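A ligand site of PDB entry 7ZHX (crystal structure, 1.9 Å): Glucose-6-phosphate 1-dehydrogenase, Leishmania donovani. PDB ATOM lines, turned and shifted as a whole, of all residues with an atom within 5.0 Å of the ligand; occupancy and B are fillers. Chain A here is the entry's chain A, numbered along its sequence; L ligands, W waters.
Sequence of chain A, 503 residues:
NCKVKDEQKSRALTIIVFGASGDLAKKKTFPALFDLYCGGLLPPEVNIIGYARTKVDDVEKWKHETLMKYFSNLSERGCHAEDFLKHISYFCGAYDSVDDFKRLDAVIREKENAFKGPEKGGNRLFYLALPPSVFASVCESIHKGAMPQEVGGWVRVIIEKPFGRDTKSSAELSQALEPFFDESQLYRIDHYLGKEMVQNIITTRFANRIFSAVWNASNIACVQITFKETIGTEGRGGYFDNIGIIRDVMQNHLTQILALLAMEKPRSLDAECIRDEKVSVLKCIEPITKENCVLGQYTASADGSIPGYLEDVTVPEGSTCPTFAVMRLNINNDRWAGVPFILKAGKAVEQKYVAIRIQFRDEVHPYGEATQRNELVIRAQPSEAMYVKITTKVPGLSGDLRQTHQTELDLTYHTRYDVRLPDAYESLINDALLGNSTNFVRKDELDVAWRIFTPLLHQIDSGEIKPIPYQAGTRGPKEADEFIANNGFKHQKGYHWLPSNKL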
ATOM      1  N   GLY A  19     -12.842  11.951   2.819  1.00  0.00           N
ATOM      2  CA  GLY A  19     -12.034  13.110   3.157  1.00  0.00           C
ATOM      3  C   GLY A  19     -11.262  12.949   4.445  1.00  0.00           C
ATOM      4  O   GLY A  19     -10.901  13.951   5.063  1.00  0.00           O
ATOM      5  N   SER A  21      -8.353  12.367   5.288  1.00  0.00           N
ATOM      6  CA  SER A  21      -7.057  13.030   5.325  1.00  0.00           C
ATOM      7  C   SER A  21      -7.143  14.490   5.707  1.00  0.00           C
ATOM      8  O   SER A  21      -6.100  15.138   5.874  1.00  0.00           O
ATOM      9  CB  SER A  21      -6.403  12.927   3.947  1.00  0.00           C
ATOM     10  OG  SER A  21      -7.290  13.500   2.974  1.00  0.00           O
ATOM     11  N   GLY A  22      -8.365  15.045   5.851  1.00  0.00           N
ATOM     12  CA  GLY A  22      -8.529  16.483   5.929  1.00  0.00           C
ATOM     13  C   GLY A  22      -8.534  17.059   7.338  1.00  0.00           C
ATOM     14  O   GLY A  22      -8.479  16.342   8.340  1.00  0.00           O
ATOM     15  N   ASP A  23      -8.608  18.385   7.380  1.00  0.00           N
ATOM     16  CA  ASP A  23      -8.572  19.144   8.636  1.00  0.00           C
ATOM     17  C   ASP A  23      -9.742  18.770   9.552  1.00  0.00           C
ATOM     18  O   ASP A  23      -9.540  18.423  10.724  1.00  0.00           O
ATOM     19  CB  ASP A  23      -8.596  20.635   8.293  1.00  0.00           C
ATOM     20  CG  ASP A  23      -8.331  21.515   9.482  1.00  0.00           C
ATOM     21  OD1 ASP A  23      -7.148  21.786   9.760  1.00  0.00           O
ATOM     22  OD2 ASP A  23      -9.320  21.943  10.127  1.00  0.00           O
ATOM     23  N   LEU A  24     -10.970  18.844   9.037  1.00  0.00           N
ATOM     24  CA  LEU A  24     -12.148  18.515   9.831  1.00  0.00           C
ATOM     25  C   LEU A  24     -12.064  17.101  10.385  1.00  0.00           C
ATOM     26  O   LEU A  24     -12.315  16.858  11.570  1.00  0.00           O
ATOM     27  CB  LEU A  24     -13.426  18.676   8.997  1.00  0.00           C
ATOM     28  CG  LEU A  24     -14.699  18.223   9.739  1.00  0.00           C
ATOM     29  CD1 LEU A  24     -15.118  19.241  10.782  1.00  0.00           C
ATOM     30  CD2 LEU A  24     -15.834  17.937   8.757  1.00  0.00           C
ATOM     31  N   ALA A  25     -11.676  16.146   9.533  1.00  0.00           N
ATOM     32  CA  ALA A  25     -11.710  14.751   9.947  1.00  0.00           C
ATOM     33  C   ALA A  25     -10.764  14.524  11.125  1.00  0.00           C
ATOM     34  O   ALA A  25     -11.138  13.895  12.122  1.00  0.00           O
ATOM     35  CB  ALA A  25     -11.341  13.842   8.772  1.00  0.00           C
ATOM     36  N   LYS A  28     -11.671  17.192  14.279  1.00  0.00           N
ATOM     37  CA  LYS A  28     -13.006  17.186  14.870  1.00  0.00           C
ATOM     38  C   LYS A  28     -13.718  15.855  14.780  1.00  0.00           C
ATOM     39  O   LYS A  28     -14.235  15.364  15.790  1.00  0.00           O
ATOM     40  CB  LYS A  28     -13.863  18.284  14.214  1.00  0.00           C
ATOM     41  CG  LYS A  28     -13.449  19.678  14.633  1.00  0.00           C
ATOM     42  CD  LYS A  28     -14.331  20.775  14.040  1.00  0.00           C
ATOM     43  CE  LYS A  28     -13.703  22.164  14.222  1.00  0.00           C
ATOM     44  NZ  LYS A  28     -14.449  23.263  13.492  1.00  0.00           N
ATOM     45  N   ALA A  52      -9.986   8.336   1.394  1.00  0.00           N
ATOM     46  CA  ALA A  52      -9.493   9.588   0.831  1.00  0.00           C
ATOM     47  C   ALA A  52      -8.507   9.261  -0.285  1.00  0.00           C
ATOM     48  O   ALA A  52      -8.074   8.115  -0.438  1.00  0.00           O
ATOM     49  CB  ALA A  52      -8.832  10.475   1.887  1.00  0.00           C
ATOM     50  N   ARG A  53      -8.136  10.282  -1.049  1.00  0.00           N
ATOM     51  CA  ARG A  53      -7.200  10.075  -2.160  1.00  0.00           C
ATOM     52  C   ARG A  53      -5.751  10.061  -1.688  1.00  0.00           C
ATOM     53  O   ARG A  53      -4.888   9.529  -2.390  1.00  0.00           O
ATOM     54  CB  ARG A  53      -7.345  11.162  -3.222  1.00  0.00           C
ATOM     55  CG  ARG A  53      -8.707  11.203  -3.942  1.00  0.00           C
ATOM     56  CD  ARG A  53      -8.876  12.540  -4.693  1.00  0.00           C
ATOM     57  NE  ARG A  53      -8.566  13.710  -3.891  1.00  0.00           N
ATOM     58  CZ  ARG A  53      -8.300  14.903  -4.416  1.00  0.00           C
ATOM     59  NH1 ARG A  53      -8.353  15.104  -5.725  1.00  0.00           N
ATOM     60  NH2 ARG A  53      -7.958  15.902  -3.612  1.00  0.00           N
ATOM     61  N   THR A  54      -5.463  10.634  -0.533  1.00  0.00           N
ATOM     62  CA  THR A  54      -4.084  10.764  -0.088  1.00  0.00           C
ATOM     63  C   THR A  54      -3.499   9.391   0.195  1.00  0.00           C
ATOM     64  O   THR A  54      -4.083   8.583   0.921  1.00  0.00           O
ATOM     65  CB  THR A  54      -4.015  11.652   1.152  1.00  0.00           C
ATOM     66  OG1 THR A  54      -4.356  12.994   0.765  1.00  0.00           O
ATOM     67  CG2 THR A  54      -2.593  11.631   1.720  1.00  0.00           C
ATOM     68  N   TYR A  90      -8.108   2.329   6.754  1.00  0.00           N
ATOM     69  CA  TYR A  90      -7.996   3.399   5.773  1.00  0.00           C
ATOM     70  C   TYR A  90      -8.047   2.805   4.380  1.00  0.00           C
ATOM     71  O   TYR A  90      -7.329   1.838   4.090  1.00  0.00           O
ATOM     72  CB  TYR A  90      -6.696   4.175   5.941  1.00  0.00           C
ATOM     73  CG  TYR A  90      -6.538   5.414   5.075  1.00  0.00           C
ATOM     74  CD1 TYR A  90      -7.102   6.629   5.448  1.00  0.00           C
ATOM     75  CD2 TYR A  90      -5.781   5.364   3.896  1.00  0.00           C
ATOM     76  CE1 TYR A  90      -6.921   7.774   4.685  1.00  0.00           C
ATOM     77  CE2 TYR A  90      -5.604   6.505   3.119  1.00  0.00           C
ATOM     78  CZ  TYR A  90      -6.179   7.703   3.518  1.00  0.00           C
ATOM     79  OH  TYR A  90      -5.975   8.842   2.773  1.00  0.00           O
ATOM     80  N   TYR A  95     -13.061   9.265  -5.219  1.00  0.00           N
ATOM     81  CA  TYR A  95     -14.480   9.526  -4.958  1.00  0.00           C
ATOM     82  C   TYR A  95     -15.352   9.290  -6.187  1.00  0.00           C
ATOM     83  O   TYR A  95     -16.572   9.163  -6.043  1.00  0.00           O
ATOM     84  CB  TYR A  95     -14.658  10.963  -4.470  1.00  0.00           C
ATOM     85  CG  TYR A  95     -13.765  11.304  -3.315  1.00  0.00           C
ATOM     86  CD1 TYR A  95     -13.848  10.622  -2.094  1.00  0.00           C
ATOM     87  CD2 TYR A  95     -12.805  12.297  -3.435  1.00  0.00           C
ATOM     88  CE1 TYR A  95     -13.015  10.937  -1.036  1.00  0.00           C
ATOM     89  CE2 TYR A  95     -11.947  12.609  -2.375  1.00  0.00           C
ATOM     90  CZ  TYR A  95     -12.075  11.929  -1.181  1.00  0.00           C
ATOM     91  OH  TYR A  95     -11.249  12.246  -0.129  1.00  0.00           O
ATOM     92  N   LEU A 128     -19.392  12.942   4.908  1.00  0.00           N
ATOM     93  CA  LEU A 128     -18.720  13.668   3.816  1.00  0.00           C
ATOM     94  C   LEU A 128     -17.867  14.799   4.399  1.00  0.00           C
ATOM     95  O   LEU A 128     -18.249  15.964   4.413  1.00  0.00           O
ATOM     96  CB  LEU A 128     -19.732  14.188   2.783  1.00  0.00           C
ATOM     97  CG  LEU A 128     -20.756  13.205   2.218  1.00  0.00           C
ATOM     98  CD1 LEU A 128     -21.463  13.746   0.942  1.00  0.00           C
ATOM     99  CD2 LEU A 128     -20.103  11.857   1.916  1.00  0.00           C
ATOM    100  N   ALA A 129     -16.664  14.446   4.870  1.00  0.00           N
ATOM    101  CA  ALA A 129     -15.741  15.475   5.365  1.00  0.00           C
ATOM    102  C   ALA A 129     -14.908  16.044   4.199  1.00  0.00           C
ATOM    103  O   ALA A 129     -13.687  16.009   4.180  1.00  0.00           O
ATOM    104  CB  ALA A 129     -14.838  14.912   6.470  1.00  0.00           C
ATOM    105  N   LEU A 130     -15.636  16.583   3.226  1.00  0.00           N
ATOM    106  CA  LEU A 130     -15.193  17.008   1.912  1.00  0.00           C
ATOM    107  C   LEU A 130     -15.735  18.394   1.611  1.00  0.00           C
ATOM    108  O   LEU A 130     -16.765  18.786   2.165  1.00  0.00           O
ATOM    109  CB  LEU A 130     -15.713  16.050   0.837  1.00  0.00           C
ATOM    110  CG  LEU A 130     -15.211  14.599   0.806  1.00  0.00           C
ATOM    111  CD1 LEU A 130     -16.103  13.810  -0.156  1.00  0.00           C
ATOM    112  CD2 LEU A 130     -13.754  14.557   0.357  1.00  0.00           C
ATOM    113  N   PRO A 131     -15.094  19.147   0.714  1.00  0.00           N
ATOM    114  CA  PRO A 131     -15.752  20.347   0.202  1.00  0.00           C
ATOM    115  C   PRO A 131     -17.028  19.972  -0.518  1.00  0.00           C
ATOM    116  O   PRO A 131     -17.126  18.897  -1.146  1.00  0.00           O
ATOM    117  CB  PRO A 131     -14.714  20.929  -0.776  1.00  0.00           C
ATOM    118  CG  PRO A 131     -13.420  20.181  -0.501  1.00  0.00           C
ATOM    119  CD  PRO A 131     -13.835  18.848   0.018  1.00  0.00           C
ATOM    120  N   PRO A 132     -18.055  20.826  -0.436  1.00  0.00           N
ATOM    121  CA  PRO A 132     -19.340  20.480  -1.069  1.00  0.00           C
ATOM    122  C   PRO A 132     -19.271  20.268  -2.570  1.00  0.00           C
ATOM    123  O   PRO A 132     -20.139  19.575  -3.120  1.00  0.00           O
ATOM    124  CB  PRO A 132     -20.238  21.676  -0.725  1.00  0.00           C
ATOM    125  CG  PRO A 132     -19.631  22.242   0.535  1.00  0.00           C
ATOM    126  CD  PRO A 132     -18.134  22.028   0.406  1.00  0.00           C
ATOM    127  N   SER A 133     -18.264  20.822  -3.255  1.00  0.00           N
ATOM    128  CA  SER A 133     -18.108  20.567  -4.698  1.00  0.00           C
ATOM    129  C   SER A 133     -17.900  19.086  -5.009  1.00  0.00           C
ATOM    130  O   SER A 133     -18.044  18.672  -6.178  1.00  0.00           O
ATOM    131  CB  SER A 133     -16.960  21.406  -5.253  1.00  0.00           C
ATOM    132  OG  SER A 133     -15.727  21.115  -4.587  1.00  0.00           O
ATOM    133  N   VAL A 134     -17.565  18.271  -4.014  1.00  0.00           N
ATOM    134  CA  VAL A 134     -17.356  16.830  -4.230  1.00  0.00           C
ATOM    135  C   VAL A 134     -18.588  16.010  -3.842  1.00  0.00           C
ATOM    136  O   VAL A 134     -18.649  14.822  -4.194  1.00  0.00           O
ATOM    137  CB  VAL A 134     -16.115  16.329  -3.447  1.00  0.00           C
ATOM    138  CG1 VAL A 134     -15.748  14.876  -3.817  1.00  0.00           C
ATOM    139  CG2 VAL A 134     -14.929  17.232  -3.700  1.00  0.00           C
ATOM    140  N   PHE A 135     -19.588  16.612  -3.191  1.00  0.00           N
ATOM    141  CA  PHE A 135     -20.722  15.842  -2.664  1.00  0.00           C
ATOM    142  C   PHE A 135     -21.450  15.055  -3.749  1.00  0.00           C
ATOM    143  O   PHE A 135     -21.753  13.874  -3.583  1.00  0.00           O
ATOM    144  CB  PHE A 135     -21.719  16.773  -1.956  1.00  0.00           C
ATOM    145  CG  PHE A 135     -21.198  17.351  -0.665  1.00  0.00           C
ATOM    146  CD1 PHE A 135     -19.993  16.913  -0.126  1.00  0.00           C
ATOM    147  CD2 PHE A 135     -21.935  18.313   0.021  1.00  0.00           C
ATOM    148  CE1 PHE A 135     -19.519  17.447   1.077  1.00  0.00           C
ATOM    149  CE2 PHE A 135     -21.473  18.842   1.223  1.00  0.00           C
ATOM    150  CZ  PHE A 135     -20.254  18.412   1.747  1.00  0.00           C
ATOM    151  N   GLU A 160     -21.834  18.085   5.060  1.00  0.00           N
ATOM    152  CA  GLU A 160     -21.213  19.231   5.711  1.00  0.00           C
ATOM    153  C   GLU A 160     -21.622  20.539   5.037  1.00  0.00           C
ATOM    154  O   GLU A 160     -22.085  20.558   3.889  1.00  0.00           O
ATOM    155  CB  GLU A 160     -19.690  19.101   5.740  1.00  0.00           C
ATOM    156  CG  GLU A 160     -19.162  18.302   6.958  1.00  0.00           C
ATOM    157  CD  GLU A 160     -19.403  19.018   8.268  1.00  0.00           C
ATOM    158  OE1 GLU A 160     -19.666  20.250   8.238  1.00  0.00           O
ATOM    159  OE2 GLU A 160     -19.338  18.369   9.330  1.00  0.00           O
ATOM    160  N   LYS A 161     -21.471  21.630   5.784  1.00  0.00           N
ATOM    161  CA  LYS A 161     -21.762  22.954   5.262  1.00  0.00           C
ATOM    162  C   LYS A 161     -20.542  23.477   4.529  1.00  0.00           C
ATOM    163  O   LYS A 161     -19.429  22.975   4.720  1.00  0.00           O
ATOM    164  CB  LYS A 161     -22.155  23.892   6.411  1.00  0.00           C
ATOM    165  CG  LYS A 161     -20.986  24.315   7.249  1.00  0.00           C
ATOM    166  CD  LYS A 161     -21.439  25.146   8.469  1.00  0.00           C
ATOM    167  CE  LYS A 161     -20.235  25.521   9.312  1.00  0.00           C
ATOM    168  NZ  LYS A 161     -19.315  26.446   8.596  1.00  0.00           N
ATOM    169  N   PRO A 162     -20.691  24.527   3.706  1.00  0.00           N
ATOM    170  CA  PRO A 162     -21.881  25.355   3.442  1.00  0.00           C
ATOM    171  C   PRO A 162     -22.923  24.652   2.583  1.00  0.00           C
ATOM    172  O   PRO A 162     -22.573  23.964   1.603  1.00  0.00           O
ATOM    173  CB  PRO A 162     -21.293  26.568   2.715  1.00  0.00           C
ATOM    174  CG  PRO A 162     -20.118  26.016   1.992  1.00  0.00           C
ATOM    175  CD  PRO A 162     -19.510  25.034   2.967  1.00  0.00           C
ATOM    176  N   HIS A 191     -23.018  21.828  13.539  1.00  0.00           N
ATOM    177  CA  HIS A 191     -22.269  21.305  14.686  1.00  0.00           C
ATOM    178  C   HIS A 191     -22.693  21.955  16.006  1.00  0.00           C
ATOM    179  O   HIS A 191     -22.399  21.420  17.082  1.00  0.00           O
ATOM    180  CB  HIS A 191     -20.767  21.573  14.529  1.00  0.00           C
ATOM    181  CG  HIS A 191     -20.094  20.779  13.438  1.00  0.00           C
ATOM    182  ND1 HIS A 191     -18.753  20.478  13.458  1.00  0.00           N
ATOM    183  CD2 HIS A 191     -20.579  20.252  12.282  1.00  0.00           C
ATOM    184  CE1 HIS A 191     -18.431  19.781  12.381  1.00  0.00           C
ATOM    185  NE2 HIS A 191     -19.523  19.642  11.639  1.00  0.00           N
HETATM  186  P1  LIG L   1     -10.360  20.283   3.280  1.00  0.00           P
HETATM  187  O1  LIG L   1      -9.983  21.373   2.334  1.00  0.00           O
HETATM  188  O2  LIG L   1      -9.300  20.032   4.275  1.00  0.00           O
HETATM  189  O3  LIG L   1     -10.746  18.883   2.480  1.00  0.00           O
HETATM  190  C1  LIG L   1     -10.918  17.705   3.220  1.00  0.00           C
HETATM  191  C2  LIG L   1     -10.416  16.589   2.302  1.00  0.00           C
HETATM  192  O4  LIG L   1     -11.158  16.515   1.210  1.00  0.00           O
HETATM  193  C3  LIG L   1      -9.008  16.992   1.785  1.00  0.00           C
HETATM  194  O5  LIG L   1      -8.049  16.531   2.689  1.00  0.00           O
HETATM  195  C4  LIG L   1      -8.969  16.242   0.471  1.00  0.00           C
HETATM  196  O6  LIG L   1      -8.619  14.833   0.824  1.00  0.00           O
HETATM  197  C5  LIG L   1     -10.230  16.262  -0.038  1.00  0.00           C
HETATM  198  N1  LIG L   1     -10.340  17.393  -0.932  1.00  0.00           N
HETATM  199  C6  LIG L   1     -10.112  18.717  -0.844  1.00  0.00           C
HETATM  200  N2  LIG L   1     -10.353  19.249  -2.051  1.00  0.00           N
HETATM  201  C7  LIG L   1     -10.734  18.259  -2.886  1.00  0.00           C
HETATM  202  C8  LIG L   1     -11.081  18.305  -4.221  1.00  0.00           C
HETATM  203  N3  LIG L   1     -11.191  19.384  -5.182  1.00  0.00           N
HETATM  204  N4  LIG L   1     -11.433  17.199  -4.868  1.00  0.00           N
HETATM  205  C9  LIG L   1     -11.436  16.015  -4.209  1.00  0.00           C
HETATM  206  N5  LIG L   1     -11.082  15.991  -2.876  1.00  0.00           N
HETATM  207  C10 LIG L   1     -10.733  17.114  -2.203  1.00  0.00           C
HETATM  208  O7  LIG L   1     -11.764  20.694   4.014  1.00  0.00           O
HETATM  209  P2  LIG L   1     -12.033  20.572   5.653  1.00  0.00           P
HETATM  210  O8  LIG L   1     -11.510  19.296   6.195  1.00  0.00           O
HETATM  211  O9  LIG L   1     -11.499  21.764   6.347  1.00  0.00           O
HETATM  212  O10 LIG L   1     -13.677  20.555   5.760  1.00  0.00           O
HETATM  213  C11 LIG L   1     -14.402  19.387   5.298  1.00  0.00           C
HETATM  214  C12 LIG L   1     -15.950  19.781   5.225  1.00  0.00           C
HETATM  215  O11 LIG L   1     -16.361  20.151   6.403  1.00  0.00           O
HETATM  216  C13 LIG L   1     -16.122  21.008   4.325  1.00  0.00           C
HETATM  217  O12 LIG L   1     -17.357  20.919   3.681  1.00  0.00           O
HETATM  218  C14 LIG L   1     -16.124  22.162   5.300  1.00  0.00           C
HETATM  219  O13 LIG L   1     -16.786  23.355   4.628  1.00  0.00           O
HETATM  220  C15 LIG L   1     -16.822  21.678   6.310  1.00  0.00           C
HETATM  221  N6  LIG L   1     -16.446  22.286   7.613  1.00  0.00           N
HETATM  222  C16 LIG L   1     -15.067  22.522   7.911  1.00  0.00           C
HETATM  223  C17 LIG L   1     -14.602  22.939   9.252  1.00  0.00           C
HETATM  224  C18 LIG L   1     -13.246  22.539   9.762  1.00  0.00           C
HETATM  225  O14 LIG L   1     -12.349  22.135   9.043  1.00  0.00           O
HETATM  226  N7  LIG L   1     -13.031  22.678  11.160  1.00  0.00           N
HETATM  227  C19 LIG L   1     -15.635  23.430  10.334  1.00  0.00           C
HETATM  228  C20 LIG L   1     -17.035  22.798  10.077  1.00  0.00           C
HETATM  229  C21 LIG L   1     -17.486  22.561   8.615  1.00  0.00           C
HETATM  230  P3  LIG L   1      -7.826  13.896  -0.318  1.00  0.00           P
HETATM  231  O15 LIG L   1      -6.967  12.966   0.491  1.00  0.00           O
HETATM  232  O16 LIG L   1      -8.868  13.106  -1.092  1.00  0.00           O
HETATM  233  O17 LIG L   1      -7.026  14.801  -1.199  1.00  0.00           O
HETATM  234  O   HOH W   1     -11.894  16.274  -7.431  1.00  0.00           O
HETATM  235  O   HOH W   2      -9.619  23.579   6.592  1.00  0.00           O
HETATM  236  O   HOH W   3     -11.686  16.544   6.598  1.00  0.00           O
HETATM  237  O   HOH W   4     -10.700  21.960  -2.566  1.00  0.00           O
HETATM  238  O   HOH W   5     -18.812  23.572  12.121  1.00  0.00           O
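NZ of Lys 28 sits close to N7 of the ligand.
Gly 19 touches the ligand.
CA of Gly 22 touches O5 of the ligand, at 3.3 Å.
Ala 52 touches the ligand.
Ala 129 touches the ligand (O to C1, 3.4 Å).
Pro 131 touches the ligand.
CD of Pro 132 touches O12 of the ligand, at 3.5 Å.
CG2 of Val 134 touches N4 of the ligand, 3.7 Å away.
Glu 160 touches the ligand.
Pro 162 touches the ligand (CD to O13, 3.6 Å).
Hydrophobic or aromatic side chains that line the ligand: Leu 24, Ala 52, Tyr 95, Leu 130, Pro 131, Pro 132, Val 134 and Pro 162.
The nearest printed residue that does not touch the ligand is His 191 (4.04 Å).
The backbone NH (N) of Gly 19 lies within hydrogen-bond range of the side-chain hydroxyl (OH) of Tyr 95, at 3.4 Å.
The side-chain hydroxyl (OH) of Tyr 90 is in hydrogen-bond range of the backbone carbonyl oxygen (O) of Thr 54.
A ring nitrogen (NE2) of His 191 sits at hydrogen-bond distance from the side-chain carboxylate (OE2) of Glu 160 (2.6 Å).
Water W3 lies within hydrogen-bond range of an oxygen (O8) of the ligand, the backbone NH of Ala 25, the backbone carbonyl oxygen of Gly 19, the backbone carbonyl oxygen of Ala 129 and the backbone NH of Leu 24.
The backbone NH (N) of Thr 54 lies within hydrogen-bond range of an oxygen (O15) of the ligand, 3.0 Å away.
O15 of the ligand lies within hydrogen-bond range of OG1 of Thr 54, 2.6 Å away.
O of Lys 161 is in hydrogen-bond range of O13 of the ligand, at 2.7 Å.
O8 of the ligand lies within hydrogen-bond range of N of Asp 23, 3.3 Å away.
The backbone NH of Leu 24 sits at hydrogen-bond distance from an oxygen (O8) of the ligand, 2.9 Å away.
The guanidinium group (NH2) of Arg 53 is in salt-bridge range of an oxygen (O17) of the ligand, at 2.8 Å.
An oxygen (O15) of the ligand is in hydrogen-bond range of the side-chain hydroxyl (OG) of Ser 21, at 2.6 Å.
The side-chain hydroxyl of Tyr 95 is in hydrogen-bond range of an oxygen (O16) of the ligand, 2.7 Å away.
The backbone carbonyl oxygen of Leu 130 is in hydrogen-bond range of an oxygen (O12) of the ligand, at 2.7 Å.
The backbone NH (N) of Arg 53 lies within hydrogen-bond range of an oxygen (O16) of the ligand (2.9 Å).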
